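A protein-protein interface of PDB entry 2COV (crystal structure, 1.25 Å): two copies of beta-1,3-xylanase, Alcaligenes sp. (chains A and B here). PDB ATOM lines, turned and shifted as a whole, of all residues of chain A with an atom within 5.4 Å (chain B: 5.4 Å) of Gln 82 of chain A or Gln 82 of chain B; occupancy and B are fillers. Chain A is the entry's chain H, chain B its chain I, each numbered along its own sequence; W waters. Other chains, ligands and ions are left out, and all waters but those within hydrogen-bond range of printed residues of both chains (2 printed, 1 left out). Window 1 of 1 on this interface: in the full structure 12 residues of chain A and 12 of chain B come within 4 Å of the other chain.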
ATOM      1  N   TRP A  32     -11.230  -3.428  25.317  1.00  0.00           N
ATOM      2  CA  TRP A  32     -11.266  -2.385  26.350  1.00  0.00           C
ATOM      3  C   TRP A  32     -12.273  -2.691  27.455  1.00  0.00           C
ATOM      4  O   TRP A  32     -13.290  -3.372  27.235  1.00  0.00           O
ATOM      5  CB  TRP A  32     -11.704  -1.081  25.742  1.00  0.00           C
ATOM      6  CG  TRP A  32     -11.016  -0.671  24.484  1.00  0.00           C
ATOM      7  CD1 TRP A  32      -9.873   0.047  24.389  1.00  0.00           C
ATOM      8  CD2 TRP A  32     -11.518  -0.807  23.162  1.00  0.00           C
ATOM      9  NE1 TRP A  32      -9.570   0.291  23.065  1.00  0.00           N
ATOM     10  CE2 TRP A  32     -10.587  -0.200  22.291  1.00  0.00           C
ATOM     11  CE3 TRP A  32     -12.649  -1.394  22.620  1.00  0.00           C
ATOM     12  CZ2 TRP A  32     -10.767  -0.157  20.936  1.00  0.00           C
ATOM     13  CZ3 TRP A  32     -12.844  -1.282  21.275  1.00  0.00           C
ATOM     14  CH2 TRP A  32     -11.889  -0.728  20.446  1.00  0.00           C
ATOM     15  N   PHE A  71     -14.888   6.976  17.397  1.00  0.00           N
ATOM     16  CA  PHE A  71     -15.173   5.965  18.420  1.00  0.00           C
ATOM     17  C   PHE A  71     -14.430   6.405  19.687  1.00  0.00           C
ATOM     18  O   PHE A  71     -13.235   6.637  19.674  1.00  0.00           O
ATOM     19  CB  PHE A  71     -14.712   4.559  18.024  1.00  0.00           C
ATOM     20  CG  PHE A  71     -15.111   3.528  19.017  1.00  0.00           C
ATOM     21  CD1 PHE A  71     -16.432   3.377  19.433  1.00  0.00           C
ATOM     22  CD2 PHE A  71     -14.170   2.760  19.665  1.00  0.00           C
ATOM     23  CE1 PHE A  71     -16.799   2.412  20.357  1.00  0.00           C
ATOM     24  CE2 PHE A  71     -14.549   1.788  20.586  1.00  0.00           C
ATOM     25  CZ  PHE A  71     -15.842   1.634  20.906  1.00  0.00           C
ATOM     26  N   LYS A  72     -15.159   6.535  20.795  1.00  0.00           N
ATOM     27  CA  LYS A  72     -14.603   6.915  22.092  1.00  0.00           C
ATOM     28  C   LYS A  72     -14.913   5.797  23.063  1.00  0.00           C
ATOM     29  O   LYS A  72     -16.059   5.341  23.133  1.00  0.00           O
ATOM     30  CB  LYS A  72     -15.326   8.212  22.608  1.00  0.00           C
ATOM     31  CG  LYS A  72     -15.485   9.319  21.676  1.00  0.00           C
ATOM     32  CD  LYS A  72     -16.134  10.511  22.410  1.00  0.00           C
ATOM     33  CE  LYS A  72     -16.378  11.616  21.444  1.00  0.00           C
ATOM     34  NZ  LYS A  72     -17.042  12.773  22.225  1.00  0.00           N
ATOM     35  N   VAL A  73     -13.930   5.379  23.854  1.00  0.00           N
ATOM     36  CA  VAL A  73     -14.190   4.241  24.722  1.00  0.00           C
ATOM     37  C   VAL A  73     -13.382   4.302  25.991  1.00  0.00           C
ATOM     38  O   VAL A  73     -12.215   4.718  26.017  1.00  0.00           O
ATOM     39  CB  VAL A  73     -13.909   2.903  23.941  1.00  0.00           C
ATOM     40  CG1 VAL A  73     -12.420   2.808  23.523  1.00  0.00           C
ATOM     41  CG2 VAL A  73     -14.356   1.666  24.710  1.00  0.00           C
ATOM     42  N   GLU A  74     -14.026   3.960  27.124  1.00  0.00           N
ATOM     43  CA  GLU A  74     -13.316   3.808  28.391  1.00  0.00           C
ATOM     44  C   GLU A  74     -12.367   2.641  28.369  1.00  0.00           C
ATOM     45  O   GLU A  74     -12.712   1.593  27.812  1.00  0.00           O
ATOM     46  CB  GLU A  74     -14.375   3.513  29.467  1.00  0.00           C
ATOM     47  CG  GLU A  74     -13.825   3.625  30.846  1.00  0.00           C
ATOM     48  CD  GLU A  74     -14.384   2.616  31.776  1.00  0.00           C
ATOM     49  OE1 GLU A  74     -15.139   3.151  32.676  1.00  0.00           O
ATOM     50  OE2 GLU A  74     -14.228   1.354  31.507  1.00  0.00           O
ATOM     51  N   ASP A  75     -11.199   2.785  28.981  1.00  0.00           N
ATOM     52  CA  ASP A  75     -10.328   1.650  29.188  1.00  0.00           C
ATOM     53  C   ASP A  75      -9.741   1.702  30.567  1.00  0.00           C
ATOM     54  O   ASP A  75      -9.893   2.687  31.304  1.00  0.00           O
ATOM     55  CB  ASP A  75      -9.293   1.471  28.086  1.00  0.00           C
ATOM     56  CG  ASP A  75      -8.743   0.039  27.976  1.00  0.00           C
ATOM     57  OD1 ASP A  75      -7.808   0.019  27.177  1.00  0.00           O
ATOM     58  OD2 ASP A  75      -9.293  -1.018  28.596  1.00  0.00           O
ATOM     59  N   GLY A  80      -8.300   5.254  31.983  1.00  0.00           N
ATOM     60  CA  GLY A  80      -7.840   5.702  30.670  1.00  0.00           C
ATOM     61  C   GLY A  80      -8.996   5.734  29.672  1.00  0.00           C
ATOM     62  O   GLY A  80     -10.151   5.430  29.975  1.00  0.00           O
ATOM     63  N   GLN A  81      -8.659   6.136  28.464  1.00  0.00           N
ATOM     64  CA  GLN A  81      -9.634   6.141  27.385  1.00  0.00           C
ATOM     65  C   GLN A  81      -8.892   6.181  26.089  1.00  0.00           C
ATOM     66  O   GLN A  81      -7.707   6.527  26.019  1.00  0.00           O
ATOM     67  CB  GLN A  81     -10.568   7.331  27.467  1.00  0.00           C
ATOM     68  CG  GLN A  81      -9.968   8.658  27.213  1.00  0.00           C
ATOM     69  CD  GLN A  81     -10.974   9.853  27.150  1.00  0.00           C
ATOM     70  OE1 GLN A  81     -10.605  10.912  26.715  1.00  0.00           O
ATOM     71  NE2 GLN A  81     -12.088   9.739  27.787  1.00  0.00           N
ATOM     72  N   GLN A  82      -9.633   5.897  25.025  1.00  0.00           N
ATOM     73  CA  GLN A  82      -9.113   6.058  23.681  1.00  0.00           C
ATOM     74  C   GLN A  82     -10.174   6.738  22.810  1.00  0.00           C
ATOM     75  O   GLN A  82     -11.350   6.392  22.941  1.00  0.00           O
ATOM     76  CB  GLN A  82      -8.830   4.700  23.058  1.00  0.00           C
ATOM     77  CG  GLN A  82      -8.051   4.670  21.728  1.00  0.00           C
ATOM     78  CD  GLN A  82      -7.438   3.329  21.366  1.00  0.00           C
ATOM     79  OE1 GLN A  82      -7.452   2.468  22.157  1.00  0.00           O
ATOM     80  NE2 GLN A  82      -6.928   3.188  20.137  1.00  0.00           N
ATOM     81  N   ILE A  83      -9.734   7.683  21.981  1.00  0.00           N
ATOM     82  CA  ILE A  83     -10.608   8.351  21.012  1.00  0.00           C
ATOM     83  C   ILE A  83      -9.947   8.200  19.659  1.00  0.00           C
ATOM     84  O   ILE A  83      -8.797   8.593  19.479  1.00  0.00           O
ATOM     85  CB  ILE A  83     -10.816   9.821  21.348  1.00  0.00           C
ATOM     86  CG1 ILE A  83     -11.489   9.940  22.709  1.00  0.00           C
ATOM     87  CG2 ILE A  83     -11.698  10.443  20.289  1.00  0.00           C
ATOM     88  CD1 ILE A  83     -11.754  11.364  23.236  1.00  0.00           C
ATOM     89  N   LEU A  84     -10.669   7.615  18.708  1.00  0.00           N
ATOM     90  CA  LEU A  84     -10.165   7.328  17.384  1.00  0.00           C
ATOM     91  C   LEU A  84     -11.085   8.067  16.379  1.00  0.00           C
ATOM     92  O   LEU A  84     -12.314   8.015  16.504  1.00  0.00           O
ATOM     93  CB  LEU A  84     -10.281   5.850  17.069  1.00  0.00           C
ATOM     94  CG  LEU A  84      -9.521   4.909  17.924  1.00  0.00           C
ATOM     95  CD1 LEU A  84     -10.472   4.234  18.869  1.00  0.00           C
ATOM     96  CD2 LEU A  84      -8.939   3.758  17.111  1.00  0.00           C
ATOM     97  N   ASP A  85     -10.492   8.755  15.409  1.00  0.00           N
ATOM     98  CA  ASP A  85     -11.245   9.438  14.370  1.00  0.00           C
ATOM     99  C   ASP A  85     -10.753   8.971  12.999  1.00  0.00           C
ATOM    100  O   ASP A  85      -9.544   8.797  12.795  1.00  0.00           O
ATOM    101  CB  ASP A  85     -10.967  10.966  14.426  1.00  0.00           C
ATOM    102  CG  ASP A  85     -11.348  11.624  15.724  1.00  0.00           C
ATOM    103  OD1 ASP A  85     -12.511  11.504  16.119  1.00  0.00           O
ATOM    104  OD2 ASP A  85     -10.478  12.291  16.341  1.00  0.00           O
ATOM    105  N   TRP B  32       0.968   3.313  12.961  1.00  0.00           N
ATOM    106  CA  TRP B  32       0.265   4.469  12.417  1.00  0.00           C
ATOM    107  C   TRP B  32       1.121   5.221  11.394  1.00  0.00           C
ATOM    108  O   TRP B  32       2.332   5.237  11.471  1.00  0.00           O
ATOM    109  CB  TRP B  32      -0.068   5.475  13.516  1.00  0.00           C
ATOM    110  CG  TRP B  32      -0.666   4.908  14.734  1.00  0.00           C
ATOM    111  CD1 TRP B  32      -1.965   4.663  14.965  1.00  0.00           C
ATOM    112  CD2 TRP B  32       0.041   4.561  15.934  1.00  0.00           C
ATOM    113  NE1 TRP B  32      -2.143   4.184  16.249  1.00  0.00           N
ATOM    114  CE2 TRP B  32      -0.928   4.113  16.871  1.00  0.00           C
ATOM    115  CE3 TRP B  32       1.383   4.639  16.327  1.00  0.00           C
ATOM    116  CZ2 TRP B  32      -0.588   3.721  18.155  1.00  0.00           C
ATOM    117  CZ3 TRP B  32       1.704   4.247  17.573  1.00  0.00           C
ATOM    118  CH2 TRP B  32       0.720   3.816  18.477  1.00  0.00           C
ATOM    119  N   PHE B  71      -0.878   9.971  24.538  1.00  0.00           N
ATOM    120  CA  PHE B  71      -0.232   9.818  23.268  1.00  0.00           C
ATOM    121  C   PHE B  71      -1.222  10.233  22.199  1.00  0.00           C
ATOM    122  O   PHE B  71      -2.347   9.688  22.152  1.00  0.00           O
ATOM    123  CB  PHE B  71       0.245   8.378  23.052  1.00  0.00           C
ATOM    124  CG  PHE B  71       1.070   8.215  21.779  1.00  0.00           C
ATOM    125  CD1 PHE B  71       2.197   8.981  21.556  1.00  0.00           C
ATOM    126  CD2 PHE B  71       0.621   7.345  20.810  1.00  0.00           C
ATOM    127  CE1 PHE B  71       2.935   8.846  20.422  1.00  0.00           C
ATOM    128  CE2 PHE B  71       1.344   7.152  19.675  1.00  0.00           C
ATOM    129  CZ  PHE B  71       2.491   7.931  19.451  1.00  0.00           C
ATOM    130  N   LYS B  72      -0.826  11.192  21.355  1.00  0.00           N
ATOM    131  CA  LYS B  72      -1.630  11.682  20.268  1.00  0.00           C
ATOM    132  C   LYS B  72      -0.886  11.367  18.986  1.00  0.00           C
ATOM    133  O   LYS B  72       0.294  11.676  18.887  1.00  0.00           O
ATOM    134  CB  LYS B  72      -1.847  13.195  20.362  1.00  0.00           C
ATOM    135  CG  LYS B  72      -2.284  13.729  21.683  1.00  0.00           C
ATOM    136  CD  LYS B  72      -2.505  15.235  21.575  1.00  0.00           C
ATOM    137  CE  LYS B  72      -2.892  15.843  22.903  1.00  0.00           C
ATOM    138  NZ  LYS B  72      -3.125  17.330  22.739  1.00  0.00           N
ATOM    139  N   VAL B  73      -1.553  10.766  18.004  1.00  0.00           N
ATOM    140  CA  VAL B  73      -0.828  10.364  16.807  1.00  0.00           C
ATOM    141  C   VAL B  73      -1.661  10.565  15.568  1.00  0.00           C
ATOM    142  O   VAL B  73      -2.850  10.233  15.503  1.00  0.00           O
ATOM    143  CB  VAL B  73      -0.289   8.939  16.968  1.00  0.00           C
ATOM    144  CG1 VAL B  73      -1.374   7.881  17.103  1.00  0.00           C
ATOM    145  CG2 VAL B  73       0.722   8.561  15.872  1.00  0.00           C
ATOM    146  N   GLU B  74      -0.991  11.074  14.523  1.00  0.00           N
ATOM    147  CA  GLU B  74      -1.583  11.204  13.196  1.00  0.00           C
ATOM    148  C   GLU B  74      -1.831   9.797  12.624  1.00  0.00           C
ATOM    149  O   GLU B  74      -0.969   8.921  12.780  1.00  0.00           O
ATOM    150  CB  GLU B  74      -0.563  11.951  12.358  1.00  0.00           C
ATOM    151  CG  GLU B  74      -1.090  12.458  11.041  1.00  0.00           C
ATOM    152  CD  GLU B  74      -1.122  11.454   9.922  1.00  0.00           C
ATOM    153  OE1 GLU B  74      -2.133  11.449   9.222  1.00  0.00           O
ATOM    154  OE2 GLU B  74      -0.131  10.697   9.750  1.00  0.00           O
ATOM    155  N   ASP B  75      -2.942   9.577  11.934  1.00  0.00           N
ATOM    156  CA  ASP B  75      -3.288   8.255  11.447  1.00  0.00           C
ATOM    157  C   ASP B  75      -3.899   8.421  10.085  1.00  0.00           C
ATOM    158  O   ASP B  75      -4.562   9.358   9.785  1.00  0.00           O
ATOM    159  CB  ASP B  75      -4.284   7.709  12.517  1.00  0.00           C
ATOM    160  CG  ASP B  75      -4.579   6.239  12.493  1.00  0.00           C
ATOM    161  OD1 ASP B  75      -5.626   5.919  13.099  1.00  0.00           O
ATOM    162  OD2 ASP B  75      -3.781   5.424  12.161  1.00  0.00           O
ATOM    163  N   GLY B  80      -7.104  10.804   9.707  1.00  0.00           N
ATOM    164  CA  GLY B  80      -7.547  10.489  11.061  1.00  0.00           C
ATOM    165  C   GLY B  80      -6.531  10.823  12.114  1.00  0.00           C
ATOM    166  O   GLY B  80      -5.467  11.409  11.849  1.00  0.00           O
ATOM    167  N   GLN B  81      -6.848  10.346  13.308  1.00  0.00           N
ATOM    168  CA  GLN B  81      -5.973  10.500  14.430  1.00  0.00           C
ATOM    169  C   GLN B  81      -6.425   9.579  15.518  1.00  0.00           C
ATOM    170  O   GLN B  81      -7.565   9.117  15.521  1.00  0.00           O
ATOM    171  CB  GLN B  81      -5.896  11.873  14.959  1.00  0.00           C
ATOM    172  CG  GLN B  81      -7.042  12.408  15.644  1.00  0.00           C
ATOM    173  CD  GLN B  81      -6.767  13.778  16.342  1.00  0.00           C
ATOM    174  OE1 GLN B  81      -6.003  14.595  15.921  1.00  0.00           O
ATOM    175  NE2 GLN B  81      -7.509  14.001  17.358  1.00  0.00           N
ATOM    176  N   GLN B  82      -5.543   9.319  16.465  1.00  0.00           N
ATOM    177  CA  GLN B  82      -5.916   8.611  17.704  1.00  0.00           C
ATOM    178  C   GLN B  82      -5.274   9.351  18.895  1.00  0.00           C
ATOM    179  O   GLN B  82      -4.181   9.880  18.812  1.00  0.00           O
ATOM    180  CB  GLN B  82      -5.352   7.207  17.699  1.00  0.00           C
ATOM    181  CG  GLN B  82      -5.918   6.372  16.591  1.00  0.00           C
ATOM    182  CD  GLN B  82      -5.530   4.924  16.673  1.00  0.00           C
ATOM    183  OE1 GLN B  82      -5.374   4.388  17.726  1.00  0.00           O
ATOM    184  NE2 GLN B  82      -5.469   4.245  15.509  1.00  0.00           N
ATOM    185  N   ILE B  83      -6.072   9.433  19.972  1.00  0.00           N
ATOM    186  CA  ILE B  83      -5.596   9.962  21.258  1.00  0.00           C
ATOM    187  C   ILE B  83      -5.880   8.932  22.338  1.00  0.00           C
ATOM    188  O   ILE B  83      -6.999   8.457  22.481  1.00  0.00           O
ATOM    189  CB  ILE B  83      -6.258  11.290  21.584  1.00  0.00           C
ATOM    190  CG1 ILE B  83      -6.033  12.324  20.477  1.00  0.00           C
ATOM    191  CG2 ILE B  83      -5.788  11.806  22.954  1.00  0.00           C
ATOM    192  CD1 ILE B  83      -6.489  13.736  20.749  1.00  0.00           C
ATOM    193  N   LEU B  84      -4.851   8.597  23.072  1.00  0.00           N
ATOM    194  CA  LEU B  84      -4.887   7.572  24.110  1.00  0.00           C
ATOM    195  C   LEU B  84      -4.426   8.198  25.401  1.00  0.00           C
ATOM    196  O   LEU B  84      -3.430   8.933  25.430  1.00  0.00           O
ATOM    197  CB  LEU B  84      -3.914   6.436  23.798  1.00  0.00           C
ATOM    198  CG  LEU B  84      -4.143   5.668  22.513  1.00  0.00           C
ATOM    199  CD1 LEU B  84      -3.215   6.099  21.476  1.00  0.00           C
ATOM    200  CD2 LEU B  84      -3.971   4.138  22.752  1.00  0.00           C
ATOM    201  N   ASP B  85      -5.207   8.006  26.468  1.00  0.00           N
ATOM    202  CA  ASP B  85      -4.841   8.563  27.793  1.00  0.00           C
ATOM    203  C   ASP B  85      -4.814   7.384  28.778  1.00  0.00           C
ATOM    204  O   ASP B  85      -5.615   6.442  28.707  1.00  0.00           O
ATOM    205  CB  ASP B  85      -5.987   9.460  28.309  1.00  0.00           C
ATOM    206  CG  ASP B  85      -6.208  10.709  27.493  1.00  0.00           C
ATOM    207  OD1 ASP B  85      -5.241  11.308  27.065  1.00  0.00           O
ATOM    208  OD2 ASP B  85      -7.363  11.126  27.356  1.00  0.00           O
HETATM  209  O   HOH W   1      -8.274   6.253  12.868  1.00  0.00           O
HETATM  210  O   HOH W   2      -8.916  11.632  18.578  1.00  0.00           O
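Of the 12 printed residues of chain A, 6 touch a printed residue of chain B. Hydrophobic or aromatic side chains of chain A within 4 Å of the printed part of chain B: Leu 84. Among the printed residues, 12 pairs touch across the chains. Among the printed residues, no Asp or Glu carboxylate lies within 4 Å of a Lys or Arg side-chain nitrogen of the other chain.
Gly 80 of chain A touches Asp 85 of chain B, and with the chains exchanged Asp 85 of chain A touches Gly 80 of chain B. Gln 82 of chain B touches its own counterpart, Gln 82 of chain A. Gln 82 of chain A touches Leu 84 of chain B, and with the chains exchanged Leu 84 of chain A touches Gln 82 of chain B. Ile 83 of chain B touches its own counterpart, Ile 83 of chain A. Positions printed for both chains: 32, 71, 72, 73, 74, 75, 80, 81, 82, 83, 84 and 85. Of the 12 pairs that touch across the chains among the printed residues, 12 have their exchanged pair printed and touching as well.
The backbone NH (N) of Val 73 of chain A lies within hydrogen-bond range of the backbone carbonyl oxygen (O) of Gln 82 of chain A, at 2.9 Å. The backbone carbonyl oxygen (O) of Phe 71 of chain B is in hydrogen-bond range of the backbone NH (N) of Leu 84 of chain B (2.9 Å). NE1 of Trp 32 of chain A lies within hydrogen-bond range of OE1 of Gln 82 of chain A (3.2 Å). The backbone carbonyl oxygen of Asp 75 of chain B sits at hydrogen-bond distance from the backbone NH of Gly 80 of chain B. N of Leu 84 of chain A sits at hydrogen-bond distance from O of Phe 71 of chain A (2.9 Å). O of Gln 82 of chain B sits at hydrogen-bond distance from N of Val 73 of chain B, at 2.9 Å.
Asp 85 of chain B touches Gly 80 of chain A (O to CA, 3.1 Å). Gln 81 of chain A touches Leu 84 of chain B (O to CA, 3.6 Å). Ile 83 of chain B touches Gln 82 of chain A (O to CA, 3.4 Å). Leu 84 of chain B touches Gln 82 of chain A. O of Ile 83 of chain A touches CA of Gln 82 of chain B, at 3.4 Å. Leu 84 of chain A touches Gln 81 of chain B (CA to O, 3.7 Å). CD of Gln 82 of chain B touches CD2 of Leu 84 of chain A, at 3.6 Å. CA of Gly 80 of chain B touches O of Asp 85 of chain A (3.1 Å).
Water W1 lies within hydrogen-bond range of the side-chain carboxylate of Asp 75 of chain B and the backbone carbonyl oxygen of Asp 85 of chain A. Water W2 lies within hydrogen-bond range of the side-chain carboxylate of Asp 85 of chain A, the side-chain amide nitrogen of Gln 81 of chain B and the backbone carbonyl oxygen of Ile 83 of chain A.
Gln 82 of chain A touches three residues of chain B. Of the printed residues of chain B, Ile 83 of chain A touches Gln 82 and Ile 83. Of the printed residues of chain B, Asp 85 of chain A touches Gly 80 and Gln 81. Of the printed residues of chain A, Gly 80 of chain B touches Asp 85 (3.1 Å). Gln 82 of chain B touches just these residues of chain A: Gln 82, Ile 83 and Leu 84. The nearest printed residue of chain A that does not touch Asp 85 of chain B is Gln 82 of chain A (5.1 Å).
The backbone carbonyl oxygen of Gln 81 of chain B lies within hydrogen-bond range of the backbone NH of Asp 85 of chain A (3.0 Å). The backbone NH (N) of Ile 83 of chain A lies within hydrogen-bond range of the backbone carbonyl oxygen (O) of Ile 83 of chain B. The backbone carbonyl oxygen (O) of Gln 81 of chain A lies within hydrogen-bond range of the backbone NH (N) of Asp 85 of chain B. NE2 of Gln 82 of chain A sits at hydrogen-bond distance from OE1 of Gln 82 of chain B (3.1 Å).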
